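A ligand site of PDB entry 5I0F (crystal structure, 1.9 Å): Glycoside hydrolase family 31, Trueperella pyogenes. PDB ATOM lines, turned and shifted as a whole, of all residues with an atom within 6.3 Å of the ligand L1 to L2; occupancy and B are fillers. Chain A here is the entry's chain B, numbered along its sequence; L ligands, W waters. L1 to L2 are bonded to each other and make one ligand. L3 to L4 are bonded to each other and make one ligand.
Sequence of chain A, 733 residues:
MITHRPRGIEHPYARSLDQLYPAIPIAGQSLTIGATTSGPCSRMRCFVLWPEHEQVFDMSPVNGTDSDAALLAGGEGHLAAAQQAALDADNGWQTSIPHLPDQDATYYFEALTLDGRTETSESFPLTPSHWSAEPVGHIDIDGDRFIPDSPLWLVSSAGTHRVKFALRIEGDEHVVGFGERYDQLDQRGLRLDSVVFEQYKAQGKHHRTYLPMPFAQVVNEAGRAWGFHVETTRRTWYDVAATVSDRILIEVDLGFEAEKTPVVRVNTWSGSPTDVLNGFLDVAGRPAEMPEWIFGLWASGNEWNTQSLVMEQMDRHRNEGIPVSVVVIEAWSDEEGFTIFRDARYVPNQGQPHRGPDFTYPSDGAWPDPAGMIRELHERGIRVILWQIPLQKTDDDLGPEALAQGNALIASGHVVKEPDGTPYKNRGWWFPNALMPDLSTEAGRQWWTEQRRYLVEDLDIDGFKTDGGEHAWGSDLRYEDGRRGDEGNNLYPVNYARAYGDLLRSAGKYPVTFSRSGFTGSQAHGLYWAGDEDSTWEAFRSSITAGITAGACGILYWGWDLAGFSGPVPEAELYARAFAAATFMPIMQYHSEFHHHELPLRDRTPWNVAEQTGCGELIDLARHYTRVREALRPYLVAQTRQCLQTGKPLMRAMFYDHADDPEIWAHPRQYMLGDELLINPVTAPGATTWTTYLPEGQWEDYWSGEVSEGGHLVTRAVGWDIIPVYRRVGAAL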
ATOM      1  N   GLY A  74     -36.873  10.572  -2.774  1.00  0.00           N
ATOM      2  CA  GLY A  74     -36.095   9.382  -2.392  1.00  0.00           C
ATOM      3  C   GLY A  74     -36.103   8.976  -0.930  1.00  0.00           C
ATOM      4  O   GLY A  74     -35.397   8.031  -0.557  1.00  0.00           O
ATOM      5  N   GLY A  77     -33.807   8.774   4.103  1.00  0.00           N
ATOM      6  CA  GLY A  77     -32.362   8.536   3.944  1.00  0.00           C
ATOM      7  C   GLY A  77     -31.638   9.548   3.045  1.00  0.00           C
ATOM      8  O   GLY A  77     -30.434   9.749   3.207  1.00  0.00           O
ATOM      9  N   HIS A  78     -32.367  10.165   2.100  1.00  0.00           N
ATOM     10  CA  HIS A  78     -31.820  11.199   1.205  1.00  0.00           C
ATOM     11  C   HIS A  78     -32.124  12.628   1.669  1.00  0.00           C
ATOM     12  O   HIS A  78     -31.956  13.563   0.892  1.00  0.00           O
ATOM     13  CB  HIS A  78     -32.345  11.029  -0.236  1.00  0.00           C
ATOM     14  CG  HIS A  78     -31.699   9.921  -0.999  1.00  0.00           C
ATOM     15  ND1 HIS A  78     -30.346   9.928  -1.318  1.00  0.00           N
ATOM     16  CD2 HIS A  78     -32.206   8.775  -1.519  1.00  0.00           C
ATOM     17  CE1 HIS A  78     -30.064   8.840  -2.008  1.00  0.00           C
ATOM     18  NE2 HIS A  78     -31.170   8.115  -2.138  1.00  0.00           N
ATOM     19  N   GLU A 198     -37.301   0.742  -4.591  1.00  0.00           N
ATOM     20  CA  GLU A 198     -36.018   1.128  -4.033  1.00  0.00           C
ATOM     21  C   GLU A 198     -36.169   1.963  -2.762  1.00  0.00           C
ATOM     22  O   GLU A 198     -36.339   3.180  -2.824  1.00  0.00           O
ATOM     23  CB  GLU A 198     -35.145   1.882  -5.046  1.00  0.00           C
ATOM     24  CG  GLU A 198     -33.715   1.990  -4.508  1.00  0.00           C
ATOM     25  CD  GLU A 198     -32.987   3.281  -4.825  1.00  0.00           C
ATOM     26  OE1 GLU A 198     -33.198   3.873  -5.906  1.00  0.00           O
ATOM     27  OE2 GLU A 198     -32.137   3.659  -3.985  1.00  0.00           O
ATOM     28  N   TYR A 200     -34.183   3.392   0.051  1.00  0.00           N
ATOM     29  CA  TYR A 200     -32.780   3.694   0.331  1.00  0.00           C
ATOM     30  C   TYR A 200     -32.598   3.726   1.843  1.00  0.00           C
ATOM     31  O   TYR A 200     -32.982   4.684   2.491  1.00  0.00           O
ATOM     32  CB  TYR A 200     -32.313   4.997  -0.332  1.00  0.00           C
ATOM     33  CG  TYR A 200     -30.912   5.464   0.047  1.00  0.00           C
ATOM     34  CD1 TYR A 200     -29.777   4.693  -0.238  1.00  0.00           C
ATOM     35  CD2 TYR A 200     -30.714   6.688   0.683  1.00  0.00           C
ATOM     36  CE1 TYR A 200     -28.499   5.129   0.117  1.00  0.00           C
ATOM     37  CE2 TYR A 200     -29.442   7.129   1.031  1.00  0.00           C
ATOM     38  CZ  TYR A 200     -28.331   6.352   0.763  1.00  0.00           C
ATOM     39  OH  TYR A 200     -27.077   6.800   1.087  1.00  0.00           O
ATOM     40  N   TRP A 429     -35.646   9.374  -8.535  1.00  0.00           N
ATOM     41  CA  TRP A 429     -34.723  10.393  -8.063  1.00  0.00           C
ATOM     42  C   TRP A 429     -33.288  10.098  -8.519  1.00  0.00           C
ATOM     43  O   TRP A 429     -32.525  11.007  -8.762  1.00  0.00           O
ATOM     44  CB  TRP A 429     -34.807  10.506  -6.516  1.00  0.00           C
ATOM     45  CG  TRP A 429     -34.580   9.200  -5.787  1.00  0.00           C
ATOM     46  CD1 TRP A 429     -33.381   8.676  -5.398  1.00  0.00           C
ATOM     47  CD2 TRP A 429     -35.584   8.237  -5.390  1.00  0.00           C
ATOM     48  NE1 TRP A 429     -33.574   7.442  -4.767  1.00  0.00           N
ATOM     49  CE2 TRP A 429     -34.917   7.161  -4.745  1.00  0.00           C
ATOM     50  CE3 TRP A 429     -36.992   8.195  -5.510  1.00  0.00           C
ATOM     51  CZ2 TRP A 429     -35.594   6.040  -4.234  1.00  0.00           C
ATOM     52  CZ3 TRP A 429     -37.672   7.068  -4.970  1.00  0.00           C
ATOM     53  CH2 TRP A 429     -36.964   6.010  -4.348  1.00  0.00           C
ATOM     54  N   TRP A 430     -32.940   8.816  -8.647  1.00  0.00           N
ATOM     55  CA  TRP A 430     -31.573   8.402  -9.059  1.00  0.00           C
ATOM     56  C   TRP A 430     -31.560   8.212 -10.572  1.00  0.00           C
ATOM     57  O   TRP A 430     -32.412   7.503 -11.112  1.00  0.00           O
ATOM     58  CB  TRP A 430     -31.266   7.086  -8.361  1.00  0.00           C
ATOM     59  CG  TRP A 430     -29.837   6.610  -8.352  1.00  0.00           C
ATOM     60  CD1 TRP A 430     -28.711   7.350  -8.137  1.00  0.00           C
ATOM     61  CD2 TRP A 430     -29.419   5.252  -8.477  1.00  0.00           C
ATOM     62  NE1 TRP A 430     -27.608   6.537  -8.164  1.00  0.00           N
ATOM     63  CE2 TRP A 430     -28.008   5.241  -8.369  1.00  0.00           C
ATOM     64  CE3 TRP A 430     -30.096   4.044  -8.695  1.00  0.00           C
ATOM     65  CZ2 TRP A 430     -27.257   4.066  -8.460  1.00  0.00           C
ATOM     66  CZ3 TRP A 430     -29.362   2.866  -8.774  1.00  0.00           C
ATOM     67  CH2 TRP A 430     -27.951   2.885  -8.658  1.00  0.00           C
ATOM     68  N   ASP A 467     -26.869  -3.599 -10.641  1.00  0.00           N
ATOM     69  CA  ASP A 467     -27.520  -2.736  -9.663  1.00  0.00           C
ATOM     70  C   ASP A 467     -28.792  -2.108 -10.262  1.00  0.00           C
ATOM     71  O   ASP A 467     -28.972  -2.092 -11.478  1.00  0.00           O
ATOM     72  CB  ASP A 467     -26.498  -1.649  -9.241  1.00  0.00           C
ATOM     73  CG  ASP A 467     -26.829  -0.952  -7.934  1.00  0.00           C
ATOM     74  OD1 ASP A 467     -27.795  -1.286  -7.238  1.00  0.00           O
ATOM     75  OD2 ASP A 467     -26.039  -0.029  -7.574  1.00  0.00           O
ATOM     76  N   GLU A 470     -35.383  -1.024 -10.428  1.00  0.00           N
ATOM     77  CA  GLU A 470     -36.661  -0.640  -9.779  1.00  0.00           C
ATOM     78  C   GLU A 470     -37.263   0.620 -10.399  1.00  0.00           C
ATOM     79  O   GLU A 470     -38.214   1.153  -9.875  1.00  0.00           O
ATOM     80  CB  GLU A 470     -36.470  -0.363  -8.284  1.00  0.00           C
ATOM     81  CG  GLU A 470     -35.562  -1.350  -7.552  1.00  0.00           C
ATOM     82  CD  GLU A 470     -34.078  -0.987  -7.542  1.00  0.00           C
ATOM     83  OE1 GLU A 470     -33.645   0.028  -8.167  1.00  0.00           O
ATOM     84  OE2 GLU A 470     -33.304  -1.734  -6.891  1.00  0.00           O
ATOM     85  N   ARG A 516     -29.632  -6.466  -6.496  1.00  0.00           N
ATOM     86  CA  ARG A 516     -30.389  -6.171  -5.280  1.00  0.00           C
ATOM     87  C   ARG A 516     -31.890  -6.316  -5.491  1.00  0.00           C
ATOM     88  O   ARG A 516     -32.604  -6.569  -4.522  1.00  0.00           O
ATOM     89  CB  ARG A 516     -30.092  -4.764  -4.729  1.00  0.00           C
ATOM     90  CG  ARG A 516     -30.515  -3.626  -5.662  1.00  0.00           C
ATOM     91  CD  ARG A 516     -30.090  -2.247  -5.168  1.00  0.00           C
ATOM     92  NE  ARG A 516     -30.782  -1.225  -5.954  1.00  0.00           N
ATOM     93  CZ  ARG A 516     -30.543   0.089  -5.901  1.00  0.00           C
ATOM     94  NH1 ARG A 516     -29.580   0.589  -5.127  1.00  0.00           N
ATOM     95  NH2 ARG A 516     -31.270   0.924  -6.618  1.00  0.00           N
ATOM     96  N   ASP A 532     -28.854  -1.300   0.285  1.00  0.00           N
ATOM     97  CA  ASP A 532     -28.164  -0.185   0.913  1.00  0.00           C
ATOM     98  C   ASP A 532     -28.574   0.008   2.360  1.00  0.00           C
ATOM     99  O   ASP A 532     -29.758   0.179   2.639  1.00  0.00           O
ATOM    100  CB  ASP A 532     -28.505   1.102   0.176  1.00  0.00           C
ATOM    101  CG  ASP A 532     -28.002   1.127  -1.231  1.00  0.00           C
ATOM    102  OD1 ASP A 532     -27.137   0.304  -1.596  1.00  0.00           O
ATOM    103  OD2 ASP A 532     -28.441   2.037  -1.974  1.00  0.00           O
ATOM    104  N   PHE A 565     -22.624  -0.045   4.411  1.00  0.00           N
ATOM    105  CA  PHE A 565     -21.778   0.640   3.444  1.00  0.00           C
ATOM    106  C   PHE A 565     -21.803   2.168   3.525  1.00  0.00           C
ATOM    107  O   PHE A 565     -20.917   2.801   2.930  1.00  0.00           O
ATOM    108  CB  PHE A 565     -22.044   0.125   2.016  1.00  0.00           C
ATOM    109  CG  PHE A 565     -22.991   0.957   1.182  1.00  0.00           C
ATOM    110  CD1 PHE A 565     -24.203   1.423   1.652  1.00  0.00           C
ATOM    111  CD2 PHE A 565     -22.703   1.163  -0.157  1.00  0.00           C
ATOM    112  CE1 PHE A 565     -25.063   2.164   0.841  1.00  0.00           C
ATOM    113  CE2 PHE A 565     -23.550   1.870  -0.976  1.00  0.00           C
ATOM    114  CZ  PHE A 565     -24.739   2.375  -0.480  1.00  0.00           C
ATOM    115  N   SER A 566     -22.786   2.733   4.225  1.00  0.00           N
ATOM    116  CA  SER A 566     -23.063   4.182   4.189  1.00  0.00           C
ATOM    117  C   SER A 566     -22.641   4.861   5.483  1.00  0.00           C
ATOM    118  O   SER A 566     -22.821   4.311   6.570  1.00  0.00           O
ATOM    119  CB  SER A 566     -24.547   4.428   3.927  1.00  0.00           C
ATOM    120  OG  SER A 566     -24.864   5.807   3.903  1.00  0.00           O
ATOM    121  N   GLU A 593     -19.968   3.010   0.243  1.00  0.00           N
ATOM    122  CA  GLU A 593     -20.671   3.981  -0.591  1.00  0.00           C
ATOM    123  C   GLU A 593     -19.759   5.127  -1.026  1.00  0.00           C
ATOM    124  O   GLU A 593     -18.846   5.526  -0.303  1.00  0.00           O
ATOM    125  CB  GLU A 593     -21.865   4.538   0.195  1.00  0.00           C
ATOM    126  CG  GLU A 593     -22.823   5.422  -0.604  1.00  0.00           C
ATOM    127  CD  GLU A 593     -24.046   5.831   0.202  1.00  0.00           C
ATOM    128  OE1 GLU A 593     -23.888   6.169   1.387  1.00  0.00           O
ATOM    129  OE2 GLU A 593     -25.162   5.815  -0.340  1.00  0.00           O
ATOM    130  N   PHE A 594     -20.053   5.684  -2.200  1.00  0.00           N
ATOM    131  CA  PHE A 594     -19.452   6.907  -2.735  1.00  0.00           C
ATOM    132  C   PHE A 594     -19.530   8.019  -1.698  1.00  0.00           C
ATOM    133  O   PHE A 594     -20.561   8.185  -1.064  1.00  0.00           O
ATOM    134  CB  PHE A 594     -20.215   7.369  -3.985  1.00  0.00           C
ATOM    135  CG  PHE A 594     -19.583   8.529  -4.704  1.00  0.00           C
ATOM    136  CD1 PHE A 594     -18.282   8.458  -5.192  1.00  0.00           C
ATOM    137  CD2 PHE A 594     -20.318   9.687  -4.948  1.00  0.00           C
ATOM    138  CE1 PHE A 594     -17.701   9.534  -5.870  1.00  0.00           C
ATOM    139  CE2 PHE A 594     -19.751  10.766  -5.627  1.00  0.00           C
ATOM    140  CZ  PHE A 594     -18.447  10.683  -6.096  1.00  0.00           C
ATOM    141  N   HIS A 595     -18.444   8.780  -1.584  1.00  0.00           N
ATOM    142  CA  HIS A 595     -18.302   9.884  -0.608  1.00  0.00           C
ATOM    143  C   HIS A 595     -17.508  11.072  -1.231  1.00  0.00           C
ATOM    144  O   HIS A 595     -16.854  11.846  -0.513  1.00  0.00           O
ATOM    145  CB  HIS A 595     -17.609   9.272   0.620  1.00  0.00           C
ATOM    146  CG  HIS A 595     -17.391  10.216   1.759  1.00  0.00           C
ATOM    147  ND1 HIS A 595     -16.173  10.317   2.401  1.00  0.00           N
ATOM    148  CD2 HIS A 595     -18.236  11.066   2.389  1.00  0.00           C
ATOM    149  CE1 HIS A 595     -16.281  11.199   3.378  1.00  0.00           C
ATOM    150  NE2 HIS A 595     -17.515  11.674   3.382  1.00  0.00           N
ATOM    151  N   HIS A 596     -17.593  11.213  -2.572  1.00  0.00           N
ATOM    152  CA  HIS A 596     -16.925  12.299  -3.317  1.00  0.00           C
ATOM    153  C   HIS A 596     -15.415  12.370  -3.063  1.00  0.00           C
ATOM    154  O   HIS A 596     -14.825  13.445  -3.149  1.00  0.00           O
ATOM    155  CB  HIS A 596     -17.607  13.657  -3.022  1.00  0.00           C
ATOM    156  CG  HIS A 596     -19.029  13.725  -3.461  1.00  0.00           C
ATOM    157  ND1 HIS A 596     -19.406  14.160  -4.718  1.00  0.00           N
ATOM    158  CD2 HIS A 596     -20.189  13.417  -2.820  1.00  0.00           C
ATOM    159  CE1 HIS A 596     -20.716  14.102  -4.844  1.00  0.00           C
ATOM    160  NE2 HIS A 596     -21.213  13.643  -3.702  1.00  0.00           N
HETATM  161  C1  LIG L   1     -26.640  10.190  -1.228  1.00  0.00           C
HETATM  162  C2  LIG L   1     -25.346   9.741  -0.541  1.00  0.00           C
HETATM  163  C3  LIG L   1     -24.221   9.597  -1.562  1.00  0.00           C
HETATM  164  C4  LIG L   1     -24.632   8.671  -2.704  1.00  0.00           C
HETATM  165  C5  LIG L   1     -25.921   9.216  -3.336  1.00  0.00           C
HETATM  166  C6  LIG L   1     -26.480   8.419  -4.525  1.00  0.00           C
HETATM  167  O1  LIG L   1     -26.475  11.517  -1.730  1.00  0.00           O
HETATM  168  O2  LIG L   1     -24.986  10.697   0.469  1.00  0.00           O
HETATM  169  O3  LIG L   1     -23.060   9.108  -0.882  1.00  0.00           O
HETATM  170  O4  LIG L   1     -23.601   8.600  -3.695  1.00  0.00           O
HETATM  171  O5  LIG L   1     -26.929   9.298  -2.311  1.00  0.00           O
HETATM  172  O6  LIG L   1     -26.366   6.989  -4.363  1.00  0.00           O
HETATM  173  C1  LG2 L   2     -27.227   6.439  -3.340  1.00  0.00           C
HETATM  174  C2  LG2 L   2     -26.855   4.969  -3.142  1.00  0.00           C
HETATM  175  C3  LG2 L   2     -27.313   4.136  -4.324  1.00  0.00           C
HETATM  176  C4  LG2 L   2     -28.813   4.303  -4.526  1.00  0.00           C
HETATM  177  C5  LG2 L   2     -29.076   5.794  -4.757  1.00  0.00           C
HETATM  178  C6  LG2 L   2     -30.536   6.117  -4.996  1.00  0.00           C
HETATM  179  O1  LG2 L   2     -25.444   4.857  -2.943  1.00  0.00           O
HETATM  180  O2  LG2 L   2     -27.004   2.748  -4.084  1.00  0.00           O
HETATM  181  O3  LG2 L   2     -29.266   3.508  -5.636  1.00  0.00           O
HETATM  182  O4  LG2 L   2     -28.619   6.577  -3.628  1.00  0.00           O
HETATM  183  O5  LG2 L   2     -31.315   5.980  -3.802  1.00  0.00           O
HETATM  184  C1  LG3 L   3     -25.850   0.088  -4.955  1.00  0.00           C
HETATM  185  C2  LG3 L   3     -24.568   0.430  -4.184  1.00  0.00           C
HETATM  186  C3  LG3 L   3     -23.566   1.065  -5.141  1.00  0.00           C
HETATM  187  C4  LG3 L   3     -24.180   2.283  -5.845  1.00  0.00           C
HETATM  188  C5  LG3 L   3     -23.230   2.762  -6.939  1.00  0.00           C
HETATM  189  C6  LG3 L   3     -26.076   0.723  -6.343  1.00  0.00           C
HETATM  190  O1  LG3 L   3     -27.003  -0.347  -4.203  1.00  0.00           O
HETATM  191  O2  LG3 L   3     -24.017  -0.742  -3.574  1.00  0.00           O
HETATM  192  O3  LG3 L   3     -22.368   1.464  -4.436  1.00  0.00           O
HETATM  193  O4  LG3 L   3     -25.481   2.029  -6.439  1.00  0.00           O
HETATM  194  O5  LG3 L   3     -23.654   4.025  -7.467  1.00  0.00           O
HETATM  195  C1  LG4 L   4     -22.636   5.031  -7.443  1.00  0.00           C
HETATM  196  C2  LG4 L   4     -23.233   6.401  -7.813  1.00  0.00           C
HETATM  197  C3  LG4 L   4     -23.540   6.489  -9.307  1.00  0.00           C
HETATM  198  C4  LG4 L   4     -22.328   6.061 -10.117  1.00  0.00           C
HETATM  199  C5  LG4 L   4     -21.885   4.665  -9.709  1.00  0.00           C
HETATM  200  C6  LG4 L   4     -20.676   4.172 -10.490  1.00  0.00           C
HETATM  201  O1  LG4 L   4     -24.427   6.642  -7.072  1.00  0.00           O
HETATM  202  O2  LG4 L   4     -23.936   7.827  -9.632  1.00  0.00           O
HETATM  203  O3  LG4 L   4     -22.661   6.092 -11.525  1.00  0.00           O
HETATM  204  O4  LG4 L   4     -21.554   4.683  -8.324  1.00  0.00           O
HETATM  205  O5  LG4 L   4     -19.545   4.979 -10.211  1.00  0.00           O
HETATM  206  O   HOH W   1     -23.737   6.042  -4.493  1.00  0.00           O
HETATM  207  O   HOH W   2     -23.608  10.494  -5.547  1.00  0.00           O
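O2 of LG2 L2 sits at hydrogen-bond distance from O4 of LG3 L3, 2.9 Å away.
O5 of LG2 L2 lies within hydrogen-bond range of OE2 of Glu 198 (2.5 Å).
OD2 of Asp 532 sits at hydrogen-bond distance from O2 of LG2 L2, 2.7 Å away.
An oxygen (O3) of LIG L1 lies within hydrogen-bond range of the backbone carbonyl oxygen of Phe 594.
A ring nitrogen (NE2) of His 78 sits at hydrogen-bond distance from an oxygen (O5) of LG2 L2.
The side-chain carboxylate of Glu 593 lies within hydrogen-bond range of an oxygen (O1) of LG2 L2 (2.8 Å).
An oxygen (O5) of LG2 L2 sits at hydrogen-bond distance from the indole nitrogen (NE1) of Trp 429, at 2.9 Å.
An oxygen (O3) of LG2 L2 sits at hydrogen-bond distance from the guanidinium group of Arg 516 (3.0 Å).
An oxygen (O1) of LG3 L3 sits at hydrogen-bond distance from the side-chain carboxylate (OD1) of Asp 532, at 2.7 Å.
The guanidinium group of Arg 516 lies within hydrogen-bond range of an oxygen (O1) of LG3 L3, 2.9 Å away.
NE1 of Trp 430 is in hydrogen-bond range of O1 of LG4 L4 (3.4 Å).
OD2 of Asp 467 is bonded to C6 of LG3 L3, at 1.4 Å.
Residues that only touch the ligand L1 to L2: Tyr 200, Trp 430 and Phe 565.
Hydrophobic or aromatic side chains within 4 Å of the ligand L1 to L2: His 78, Tyr 200, Trp 429, Trp 430, Phe 565 and Phe 594.
Ten residues have an atom within 4 Å of the ligand L1 to L2: His 78, Glu 198, Tyr 200, Trp 429, Trp 430, Arg 516, Asp 532, Phe 565, Glu 593 and Phe 594.
The nearest printed residue that does not touch the ligand L1 to L2 is Asp 467 (4.6 Å).
NH2 of Arg 516 lies within salt-bridge range of OE1 of Glu 198 (3.6 Å).
OD2 of Asp 532 lies within salt-bridge range of NH1 of Arg 516 (3.7 Å).
N of Glu 593 sits at hydrogen-bond distance from O of Phe 565 (2.9 Å).
The side-chain carboxylate (OE2) of Glu 593 sits at hydrogen-bond distance from the side-chain hydroxyl (OH) of Tyr 200.
OE1 of Glu 593 sits at hydrogen-bond distance from OG of Ser 566.
The side-chain carboxylate (OD1) of Asp 467 lies within salt-bridge range of the guanidinium group (NE) of Arg 516 (3.3 Å).
OE2 of Glu 470 is in salt-bridge range of NE of Arg 516 (2.7 Å).
Water W1 bridges O1 of LG2 L2 (2.6 Å) and O1 of LG4 L4 (2.7 Å).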
